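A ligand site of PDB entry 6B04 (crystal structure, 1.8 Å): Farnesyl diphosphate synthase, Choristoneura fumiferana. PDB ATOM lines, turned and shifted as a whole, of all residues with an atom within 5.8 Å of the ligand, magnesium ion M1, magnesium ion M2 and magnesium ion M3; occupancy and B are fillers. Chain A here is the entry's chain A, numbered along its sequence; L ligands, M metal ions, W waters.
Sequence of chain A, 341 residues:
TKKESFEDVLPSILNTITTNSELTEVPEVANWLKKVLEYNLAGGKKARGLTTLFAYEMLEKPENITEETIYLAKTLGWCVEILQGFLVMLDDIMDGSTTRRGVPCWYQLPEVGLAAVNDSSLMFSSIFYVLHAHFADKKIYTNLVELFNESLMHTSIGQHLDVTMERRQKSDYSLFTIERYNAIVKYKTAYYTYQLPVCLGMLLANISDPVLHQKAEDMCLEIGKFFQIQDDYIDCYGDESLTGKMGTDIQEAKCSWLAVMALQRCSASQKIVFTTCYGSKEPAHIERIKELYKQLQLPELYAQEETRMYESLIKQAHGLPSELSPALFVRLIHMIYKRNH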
ATOM      1  N   LEU A  87     -32.154  -2.439   1.822  1.00  0.00           N
ATOM      2  CA  LEU A  87     -31.652  -2.415   3.227  1.00  0.00           C
ATOM      3  C   LEU A  87     -30.192  -2.624   3.306  1.00  0.00           C
ATOM      4  O   LEU A  87     -29.486  -1.875   4.001  1.00  0.00           O
ATOM      5  CB  LEU A  87     -32.342  -3.448   4.101  1.00  0.00           C
ATOM      6  CG  LEU A  87     -33.822  -3.230   4.349  1.00  0.00           C
ATOM      7  CD1 LEU A  87     -34.356  -4.515   4.997  1.00  0.00           C
ATOM      8  CD2 LEU A  87     -34.120  -2.032   5.205  1.00  0.00           C
ATOM      9  N   VAL A  88     -29.676  -3.611   2.609  1.00  0.00           N
ATOM     10  CA  VAL A  88     -28.229  -3.862   2.648  1.00  0.00           C
ATOM     11  C   VAL A  88     -27.335  -2.881   1.889  1.00  0.00           C
ATOM     12  O   VAL A  88     -26.164  -2.651   2.243  1.00  0.00           O
ATOM     13  CB  VAL A  88     -27.765  -5.342   2.420  1.00  0.00           C
ATOM     14  CG1 VAL A  88     -28.440  -6.284   3.395  1.00  0.00           C
ATOM     15  CG2 VAL A  88     -27.921  -5.822   0.986  1.00  0.00           C
ATOM     16  N   ASP A  91     -27.073  -0.387   4.634  1.00  0.00           N
ATOM     17  CA  ASP A  91     -26.328  -1.033   5.767  1.00  0.00           C
ATOM     18  C   ASP A  91     -24.857  -1.065   5.505  1.00  0.00           C
ATOM     19  O   ASP A  91     -24.077  -0.777   6.408  1.00  0.00           O
ATOM     20  CB  ASP A  91     -26.840  -2.424   5.946  1.00  0.00           C
ATOM     21  CG  ASP A  91     -26.135  -3.135   7.134  1.00  0.00           C
ATOM     22  OD1 ASP A  91     -26.536  -2.821   8.276  1.00  0.00           O
ATOM     23  OD2 ASP A  91     -25.333  -3.959   6.814  1.00  0.00           O
ATOM     24  N   ASP A  92     -24.445  -1.416   4.274  1.00  0.00           N
ATOM     25  CA  ASP A  92     -23.075  -1.441   3.925  1.00  0.00           C
ATOM     26  C   ASP A  92     -22.369  -0.094   4.076  1.00  0.00           C
ATOM     27  O   ASP A  92     -21.200  -0.011   4.523  1.00  0.00           O
ATOM     28  CB  ASP A  92     -22.838  -2.035   2.533  1.00  0.00           C
ATOM     29  CG  ASP A  92     -23.004  -3.564   2.491  1.00  0.00           C
ATOM     30  OD1 ASP A  92     -22.898  -4.221   3.551  1.00  0.00           O
ATOM     31  OD2 ASP A  92     -23.313  -4.167   1.431  1.00  0.00           O
ATOM     32  N   ASP A  95     -22.102   0.508   7.923  1.00  0.00           N
ATOM     33  CA  ASP A  95     -21.243  -0.537   8.584  1.00  0.00           C
ATOM     34  C   ASP A  95     -19.819  -0.483   8.142  1.00  0.00           C
ATOM     35  O   ASP A  95     -18.983  -1.252   8.642  1.00  0.00           O
ATOM     36  CB  ASP A  95     -21.863  -1.944   8.447  1.00  0.00           C
ATOM     37  CG  ASP A  95     -23.145  -2.080   9.219  1.00  0.00           C
ATOM     38  OD1 ASP A  95     -23.508  -1.105  10.015  1.00  0.00           O
ATOM     39  OD2 ASP A  95     -23.914  -3.109   9.158  1.00  0.00           O
ATOM     40  N   SER A  97     -18.669  -1.465   5.308  1.00  0.00           N
ATOM     41  CA  SER A  97     -18.361  -2.698   4.650  1.00  0.00           C
ATOM     42  C   SER A  97     -17.668  -2.446   3.303  1.00  0.00           C
ATOM     43  O   SER A  97     -17.717  -1.374   2.800  1.00  0.00           O
ATOM     44  CB  SER A  97     -19.596  -3.608   4.615  1.00  0.00           C
ATOM     45  OG  SER A  97     -20.053  -3.871   5.985  1.00  0.00           O
ATOM     46  N   ARG A 100     -19.611  -7.598  -0.521  1.00  0.00           N
ATOM     47  CA  ARG A 100     -20.804  -8.361  -0.309  1.00  0.00           C
ATOM     48  C   ARG A 100     -21.035  -9.239  -1.583  1.00  0.00           C
ATOM     49  O   ARG A 100     -20.687  -8.808  -2.701  1.00  0.00           O
ATOM     50  CB  ARG A 100     -22.044  -7.469  -0.104  1.00  0.00           C
ATOM     51  CG  ARG A 100     -23.210  -8.352   0.279  1.00  0.00           C
ATOM     52  CD  ARG A 100     -24.460  -7.669   0.625  1.00  0.00           C
ATOM     53  NE  ARG A 100     -24.303  -6.871   1.827  1.00  0.00           N
ATOM     54  CZ  ARG A 100     -24.640  -7.296   3.049  1.00  0.00           C
ATOM     55  NH1 ARG A 100     -25.067  -8.504   3.250  1.00  0.00           N
ATOM     56  NH2 ARG A 100     -24.511  -6.487   4.089  1.00  0.00           N
ATOM     57  N   THR A 155     -37.617  -2.244  10.442  1.00  0.00           N
ATOM     58  CA  THR A 155     -36.240  -2.348  10.200  1.00  0.00           C
ATOM     59  C   THR A 155     -35.414  -1.124  10.559  1.00  0.00           C
ATOM     60  O   THR A 155     -34.322  -1.231  11.096  1.00  0.00           O
ATOM     61  CB  THR A 155     -35.928  -2.831   8.733  1.00  0.00           C
ATOM     62  OG1 THR A 155     -36.742  -3.977   8.391  1.00  0.00           O
ATOM     63  CG2 THR A 155     -34.591  -3.212   8.596  1.00  0.00           C
ATOM     64  N   GLN A 159     -32.320  -0.669  13.009  1.00  0.00           N
ATOM     65  CA  GLN A 159     -31.085  -0.086  12.539  1.00  0.00           C
ATOM     66  C   GLN A 159     -30.677   1.106  13.407  1.00  0.00           C
ATOM     67  O   GLN A 159     -29.484   1.304  13.633  1.00  0.00           O
ATOM     68  CB  GLN A 159     -31.154   0.409  11.101  1.00  0.00           C
ATOM     69  CG  GLN A 159     -31.192  -0.763  10.138  1.00  0.00           C
ATOM     70  CD  GLN A 159     -29.931  -1.583  10.062  1.00  0.00           C
ATOM     71  OE1 GLN A 159     -29.660  -2.393  10.968  1.00  0.00           O
ATOM     72  NE2 GLN A 159     -29.146  -1.407   8.991  1.00  0.00           N
ATOM     73  N   ASP A 162     -29.050  -0.315  16.411  1.00  0.00           N
ATOM     74  CA  ASP A 162     -27.785  -0.911  15.991  1.00  0.00           C
ATOM     75  C   ASP A 162     -26.657   0.058  15.796  1.00  0.00           C
ATOM     76  O   ASP A 162     -25.540  -0.217  16.199  1.00  0.00           O
ATOM     77  CB  ASP A 162     -28.054  -1.741  14.694  1.00  0.00           C
ATOM     78  CG  ASP A 162     -26.786  -2.363  14.096  1.00  0.00           C
ATOM     79  OD1 ASP A 162     -25.976  -1.594  13.493  1.00  0.00           O
ATOM     80  OD2 ASP A 162     -26.688  -3.629  14.205  1.00  0.00           O
ATOM     81  N   VAL A 163     -26.931   1.216  15.154  1.00  0.00           N
ATOM     82  CA  VAL A 163     -25.855   2.039  14.630  1.00  0.00           C
ATOM     83  C   VAL A 163     -25.735   3.242  15.584  1.00  0.00           C
ATOM     84  O   VAL A 163     -24.819   3.985  15.443  1.00  0.00           O
ATOM     85  CB  VAL A 163     -26.081   2.636  13.223  1.00  0.00           C
ATOM     86  CG1 VAL A 163     -26.233   1.535  12.185  1.00  0.00           C
ATOM     87  CG2 VAL A 163     -27.319   3.534  13.204  1.00  0.00           C
ATOM     88  N   LYS A 188     -34.446  -5.151  13.652  1.00  0.00           N
ATOM     89  CA  LYS A 188     -33.643  -4.950  12.445  1.00  0.00           C
ATOM     90  C   LYS A 188     -33.729  -6.180  11.518  1.00  0.00           C
ATOM     91  O   LYS A 188     -33.497  -6.039  10.324  1.00  0.00           O
ATOM     92  CB  LYS A 188     -32.179  -4.643  12.689  1.00  0.00           C
ATOM     93  CG  LYS A 188     -31.277  -5.793  13.046  1.00  0.00           C
ATOM     94  CD  LYS A 188     -29.842  -5.375  13.014  1.00  0.00           C
ATOM     95  CE  LYS A 188     -28.912  -6.464  13.538  1.00  0.00           C
ATOM     96  NZ  LYS A 188     -27.489  -6.270  13.287  1.00  0.00           N
ATOM     97  N   THR A 189     -33.979  -7.347  12.126  1.00  0.00           N
ATOM     98  CA  THR A 189     -33.869  -8.620  11.325  1.00  0.00           C
ATOM     99  C   THR A 189     -35.108  -9.434  11.299  1.00  0.00           C
ATOM    100  O   THR A 189     -35.508  -9.853  10.199  1.00  0.00           O
ATOM    101  CB  THR A 189     -32.731  -9.495  11.813  1.00  0.00           C
ATOM    102  OG1 THR A 189     -31.527  -8.837  11.529  1.00  0.00           O
ATOM    103  CG2 THR A 189     -32.667 -10.850  11.156  1.00  0.00           C
ATOM    104  N   TYR A 192     -38.350  -8.366   8.799  1.00  0.00           N
ATOM    105  CA  TYR A 192     -38.268  -8.492   7.368  1.00  0.00           C
ATOM    106  C   TYR A 192     -37.784  -9.836   6.883  1.00  0.00           C
ATOM    107  O   TYR A 192     -38.112 -10.221   5.773  1.00  0.00           O
ATOM    108  CB  TYR A 192     -37.448  -7.372   6.704  1.00  0.00           C
ATOM    109  CG  TYR A 192     -36.001  -7.628   6.528  1.00  0.00           C
ATOM    110  CD1 TYR A 192     -35.132  -7.351   7.557  1.00  0.00           C
ATOM    111  CD2 TYR A 192     -35.511  -8.207   5.410  1.00  0.00           C
ATOM    112  CE1 TYR A 192     -33.801  -7.576   7.441  1.00  0.00           C
ATOM    113  CE2 TYR A 192     -34.170  -8.436   5.253  1.00  0.00           C
ATOM    114  CZ  TYR A 192     -33.327  -8.107   6.271  1.00  0.00           C
ATOM    115  OH  TYR A 192     -31.985  -8.292   6.153  1.00  0.00           O
ATOM    116  N   THR A 193     -37.004 -10.543   7.709  1.00  0.00           N
ATOM    117  CA  THR A 193     -36.454 -11.836   7.340  1.00  0.00           C
ATOM    118  C   THR A 193     -37.483 -12.968   7.416  1.00  0.00           C
ATOM    119  O   THR A 193     -37.407 -13.820   6.586  1.00  0.00           O
ATOM    120  CB  THR A 193     -35.166 -12.092   8.155  1.00  0.00           C
ATOM    121  OG1 THR A 193     -34.263 -11.039   7.830  1.00  0.00           O
ATOM    122  CG2 THR A 193     -34.435 -13.266   7.730  1.00  0.00           C
ATOM    123  N   GLN A 228     -30.238 -14.098  13.464  1.00  0.00           N
ATOM    124  CA  GLN A 228     -29.277 -13.018  13.619  1.00  0.00           C
ATOM    125  C   GLN A 228     -28.117 -13.389  14.546  1.00  0.00           C
ATOM    126  O   GLN A 228     -27.009 -12.913  14.394  1.00  0.00           O
ATOM    127  CB  GLN A 228     -29.952 -11.724  14.153  1.00  0.00           C
ATOM    128  CG  GLN A 228     -29.021 -10.535  14.144  1.00  0.00           C
ATOM    129  CD  GLN A 228     -28.480 -10.232  12.818  1.00  0.00           C
ATOM    130  OE1 GLN A 228     -29.261 -10.243  11.817  1.00  0.00           O
ATOM    131  NE2 GLN A 228     -27.205  -9.934  12.722  1.00  0.00           N
ATOM    132  N   ASP A 231     -25.909 -14.950  12.121  1.00  0.00           N
ATOM    133  CA  ASP A 231     -25.242 -13.890  11.354  1.00  0.00           C
ATOM    134  C   ASP A 231     -24.061 -13.300  12.138  1.00  0.00           C
ATOM    135  O   ASP A 231     -22.973 -13.039  11.635  1.00  0.00           O
ATOM    136  CB  ASP A 231     -26.257 -12.805  10.957  1.00  0.00           C
ATOM    137  CG  ASP A 231     -25.658 -11.800  10.042  1.00  0.00           C
ATOM    138  OD1 ASP A 231     -25.287 -12.221   8.897  1.00  0.00           O
ATOM    139  OD2 ASP A 231     -25.406 -10.615  10.469  1.00  0.00           O
ATOM    140  N   ASP A 232     -24.313 -13.039  13.422  1.00  0.00           N
ATOM    141  CA  ASP A 232     -23.249 -12.388  14.232  1.00  0.00           C
ATOM    142  C   ASP A 232     -22.029 -13.344  14.443  1.00  0.00           C
ATOM    143  O   ASP A 232     -20.877 -12.968  14.304  1.00  0.00           O
ATOM    144  CB  ASP A 232     -23.812 -12.050  15.624  1.00  0.00           C
ATOM    145  CG  ASP A 232     -24.762 -10.848  15.633  1.00  0.00           C
ATOM    146  OD1 ASP A 232     -24.892 -10.199  14.590  1.00  0.00           O
ATOM    147  OD2 ASP A 232     -25.321 -10.574  16.726  1.00  0.00           O
ATOM    148  N   ASP A 235     -20.016 -13.408  11.326  1.00  0.00           N
ATOM    149  CA  ASP A 235     -19.230 -12.217  11.062  1.00  0.00           C
ATOM    150  C   ASP A 235     -17.812 -12.422  11.518  1.00  0.00           C
ATOM    151  O   ASP A 235     -16.830 -11.957  10.906  1.00  0.00           O
ATOM    152  CB  ASP A 235     -19.833 -10.996  11.781  1.00  0.00           C
ATOM    153  CG  ASP A 235     -19.249  -9.680  11.264  1.00  0.00           C
ATOM    154  OD1 ASP A 235     -19.671  -9.320  10.186  1.00  0.00           O
ATOM    155  OD2 ASP A 235     -18.310  -9.102  11.848  1.00  0.00           O
ATOM    156  N   LYS A 245     -18.381 -11.767   2.243  1.00  0.00           N
ATOM    157  CA  LYS A 245     -18.297 -10.440   2.873  1.00  0.00           C
ATOM    158  C   LYS A 245     -17.275 -10.495   3.999  1.00  0.00           C
ATOM    159  O   LYS A 245     -17.170 -11.481   4.716  1.00  0.00           O
ATOM    160  CB  LYS A 245     -19.650  -9.932   3.381  1.00  0.00           C
ATOM    161  CG  LYS A 245     -20.444 -10.892   4.202  1.00  0.00           C
ATOM    162  CD  LYS A 245     -21.834 -10.365   4.620  1.00  0.00           C
ATOM    163  CE  LYS A 245     -22.255 -10.826   6.024  1.00  0.00           C
ATOM    164  NZ  LYS A 245     -23.686 -11.229   6.222  1.00  0.00           N
ATOM    165  N   THR A 248     -17.223  -6.832   9.899  1.00  0.00           N
ATOM    166  CA  THR A 248     -16.798  -5.586  10.451  1.00  0.00           C
ATOM    167  C   THR A 248     -17.356  -5.340  11.866  1.00  0.00           C
ATOM    168  O   THR A 248     -17.172  -4.244  12.404  1.00  0.00           O
ATOM    169  CB  THR A 248     -17.248  -4.358   9.577  1.00  0.00           C
ATOM    170  OG1 THR A 248     -18.674  -4.390   9.482  1.00  0.00           O
ATOM    171  CG2 THR A 248     -16.530  -4.340   8.194  1.00  0.00           C
ATOM    172  N   ASP A 249     -18.035  -6.337  12.461  1.00  0.00           N
ATOM    173  CA  ASP A 249     -18.698  -6.098  13.715  1.00  0.00           C
ATOM    174  C   ASP A 249     -17.711  -5.630  14.831  1.00  0.00           C
ATOM    175  O   ASP A 249     -18.047  -4.739  15.633  1.00  0.00           O
ATOM    176  CB  ASP A 249     -19.463  -7.280  14.247  1.00  0.00           C
ATOM    177  CG  ASP A 249     -20.745  -7.614  13.447  1.00  0.00           C
ATOM    178  OD1 ASP A 249     -21.124  -6.744  12.607  1.00  0.00           O
ATOM    179  OD2 ASP A 249     -21.361  -8.681  13.695  1.00  0.00           O
ATOM    180  N   LYS A 254     -19.933  -3.190  17.340  1.00  0.00           N
ATOM    181  CA  LYS A 254     -21.339  -3.579  17.348  1.00  0.00           C
ATOM    182  C   LYS A 254     -21.716  -4.355  18.619  1.00  0.00           C
ATOM    183  O   LYS A 254     -20.878  -5.117  19.183  1.00  0.00           O
ATOM    184  CB  LYS A 254     -21.683  -4.519  16.167  1.00  0.00           C
ATOM    185  CG  LYS A 254     -21.633  -3.867  14.778  1.00  0.00           C
ATOM    186  CD  LYS A 254     -22.611  -2.686  14.577  1.00  0.00           C
ATOM    187  CE  LYS A 254     -22.428  -2.114  13.129  1.00  0.00           C
ATOM    188  NZ  LYS A 254     -23.356  -1.054  12.784  1.00  0.00           N
HETATM  189  O1  LIG L   1     -24.892  -7.503  10.595  1.00  0.00           O
HETATM  190  P1  LIG L   1     -25.998  -6.699   9.809  1.00  0.00           P
HETATM  191  O2  LIG L   1     -25.303  -5.396   9.348  1.00  0.00           O
HETATM  192  O3  LIG L   1     -27.255  -6.569  10.595  1.00  0.00           O
HETATM  193  C1  LIG L   1     -26.370  -7.735   8.280  1.00  0.00           C
HETATM  194  P2  LIG L   1     -24.813  -8.088   7.427  1.00  0.00           P
HETATM  195  O4  LIG L   1     -25.324  -8.782   6.029  1.00  0.00           O
HETATM  196  O5  LIG L   1     -24.022  -6.778   7.004  1.00  0.00           O
HETATM  197  O6  LIG L   1     -23.938  -9.040   8.179  1.00  0.00           O
HETATM  198  C2  LIG L   1     -27.355  -7.021   7.351  1.00  0.00           C
HETATM  199  C3  LIG L   1     -28.615  -6.475   7.852  1.00  0.00           C
HETATM  200  C4  LIG L   1     -28.878  -5.136   7.533  1.00  0.00           C
HETATM  201  C5  LIG L   1     -30.005  -4.496   7.959  1.00  0.00           C
HETATM  202  C6  LIG L   1     -30.832  -5.176   8.762  1.00  0.00           C
HETATM  203  C7  LIG L   1     -30.642  -6.517   9.087  1.00  0.00           C
HETATM  204  N1  LIG L   1     -29.531  -7.141   8.612  1.00  0.00           N
HETATM  205  C8  LIG L   1     -29.324  -8.532   8.999  1.00  0.00           C
HETATM  206 MG    MG M   1     -25.719  -3.463  10.068  1.00  0.00          MG
HETATM  207 MG    MG M   2     -23.907  -4.985   7.944  1.00  0.00          MG
HETATM  208 MG    MG M   3     -23.879  -9.243  10.237  1.00  0.00          MG
HETATM  209  O   HOH W   1     -27.492  -3.957  10.748  1.00  0.00           O
HETATM  210  O   HOH W   2     -23.893  -6.272  12.683  1.00  0.00           O
HETATM  211  O   HOH W   3     -29.114 -11.619   9.301  1.00  0.00           O
HETATM  212  O   HOH W   4     -22.522 -10.984   9.818  1.00  0.00           O
HETATM  213  O   HOH W   5     -22.597  -4.334   6.388  1.00  0.00           O
HETATM  214  O   HOH W   6     -22.060  -8.118  10.259  1.00  0.00           O
HETATM  215  O   HOH W   7     -25.987  -1.450  10.712  1.00  0.00           O
HETATM  216  O   HOH W   8     -24.759  -3.862  11.969  1.00  0.00           O
HETATM  217  O   HOH W   9     -21.528  -7.378   6.128  1.00  0.00           O
HETATM  218  O   HOH W  10     -28.101 -10.021   5.179  1.00  0.00           O
HETATM  219  O   HOH W  11     -22.280  -5.609   9.013  1.00  0.00           O
HETATM  220  O   HOH W  12     -23.490  -9.529  12.339  1.00  0.00           O
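O4 of the ligand lies within salt-bridge range of NZ of Lys 245, at 3.0 Å.
An oxygen (O4) of the ligand lies within salt-bridge range of the guanidinium group of Arg 100, 2.8 Å away.
The side-chain amino group of Lys 188 is in salt-bridge range of an oxygen (O3) of the ligand, 2.7 Å away.
The side-chain carboxylate (OD1) of Asp 91 sits close to the side-chain amide nitrogen (NE2) of Gln 159 (3.1 Å).
The side-chain amide oxygen (OE1) of Gln 228 lies within hydrogen-bond range of the side-chain hydroxyl (OG1) of Thr 189 (2.7 Å).
The guanidinium group (NH2) of Arg 100 is in salt-bridge range of the side-chain carboxylate (OD1) of Asp 92, 2.8 Å away.
The side-chain carboxylate of Asp 91 lies close to the guanidinium group of Arg 100 (3.8 Å).
OD2 of Asp 231 lies close to NE2 of Gln 228, at 3.0 Å.
NZ of Lys 188 lies within salt-bridge range of OD2 of Asp 162.
The backbone carbonyl oxygen of Asp 95 sits at hydrogen-bond distance from the side-chain hydroxyl of Thr 248 (3.3 Å).
The side-chain amide nitrogen of Gln 228 sits at hydrogen-bond distance from the side-chain carboxylate of Asp 232, 3.0 Å away.
Gln 159 touches the ligand (NE2 to C5, 3.4 Å).
Thr 189 touches the ligand (OG1 to C8, 3.4 Å).
Tyr 192 touches the ligand.
Gln 228 touches the ligand.
Hydrophobic or aromatic side chains within 4 Å of the ligand: Tyr 192.
Ten residues have an atom within 4 Å of the ligand: Asp 91, Asp 95, Arg 100, Gln 159, Lys 188, Thr 189, Tyr 192, Gln 228, Asp 231 and Lys 245.
The nearest printed residue that does not touch the ligand is Val 88 (4.2 Å).
Asp 162 touches magnesium ion M1 (OD1 to MG, 3.9 Å).
Of the 23 residues printed, 3 come within 4 Å of magnesium ion M1.
Along chain A the residues within 4 Å of magnesium ion M1 span positions 91 to 162.
The nearest printed residue that does not touch magnesium ion M1 is Gln 159 (4.1 Å).
Within 4 Å of magnesium ion M2: Asp 91 and Asp 95.
Within 4 Å of magnesium ion M3: Asp 231.
The nearest printed residue that does not touch magnesium ion M3 is Gln 228 (4.2 Å).
Magnesium ion M1 is bound by water W1 (2.0 Å), OD2 of Asp 95 (2.1 Å), OD1 of Asp 91 (2.1 Å), O2 of the ligand (2.1 Å), water W7 (2.1 Å) and water W8 (2.2 Å).
Magnesium ion M1 has six donor atoms within binding distance.
Magnesium ion M2 is bound by an oxygen (O2) of the ligand, at 2.0 Å.
Magnesium ion M2 is bound by O5 of the ligand, 2.0 Å away.
Magnesium ion M2 is bound by water W11, at 2.0 Å.
Magnesium ion M2 is bound by OD2 of Asp 91, at 2.1 Å.
Magnesium ion M2 is bound by water W5, at 2.1 Å.
Magnesium ion M2 is bound by OD2 of Asp 95, 2.2 Å away.
Magnesium ion M3 is bound by O1 of the ligand (2.0 Å), OD2 of Asp 231 (2.1 Å), O6 of the ligand (2.1 Å), water W6 (2.1 Å), water W12 (2.2 Å) and water W4 (2.2 Å).
Water W8 bridges the side-chain carboxylate (OD2) of Asp 162 (3.0 Å) and the side-chain amino group (NZ) of Lys 254 (3.2 Å).
Water W7 lies within hydrogen-bond range of OD1 of Asp 95 (2.6 Å), OD1 of Asp 162 (2.8 Å) and NZ of Lys 254 (3.4 Å).
Water W1 lies within hydrogen-bond range of an oxygen (O3) of the ligand (2.6 Å), the side-chain amide oxygen of Gln 159 (2.7 Å) and the side-chain amino group of Lys 188 (3.4 Å).
Water W12 bridges the side-chain carboxylate (OD2) of Asp 249 and the side-chain carboxylate (OD1) of Asp 232.
Water W6 lies within hydrogen-bond range of OD1 of Asp 235 (2.7 Å) and OD1 of Asp 249 (2.9 Å).
Water W4 lies within hydrogen-bond range of O of Asp 231 (2.8 Å) and OD1 of Asp 235 (3.3 Å).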
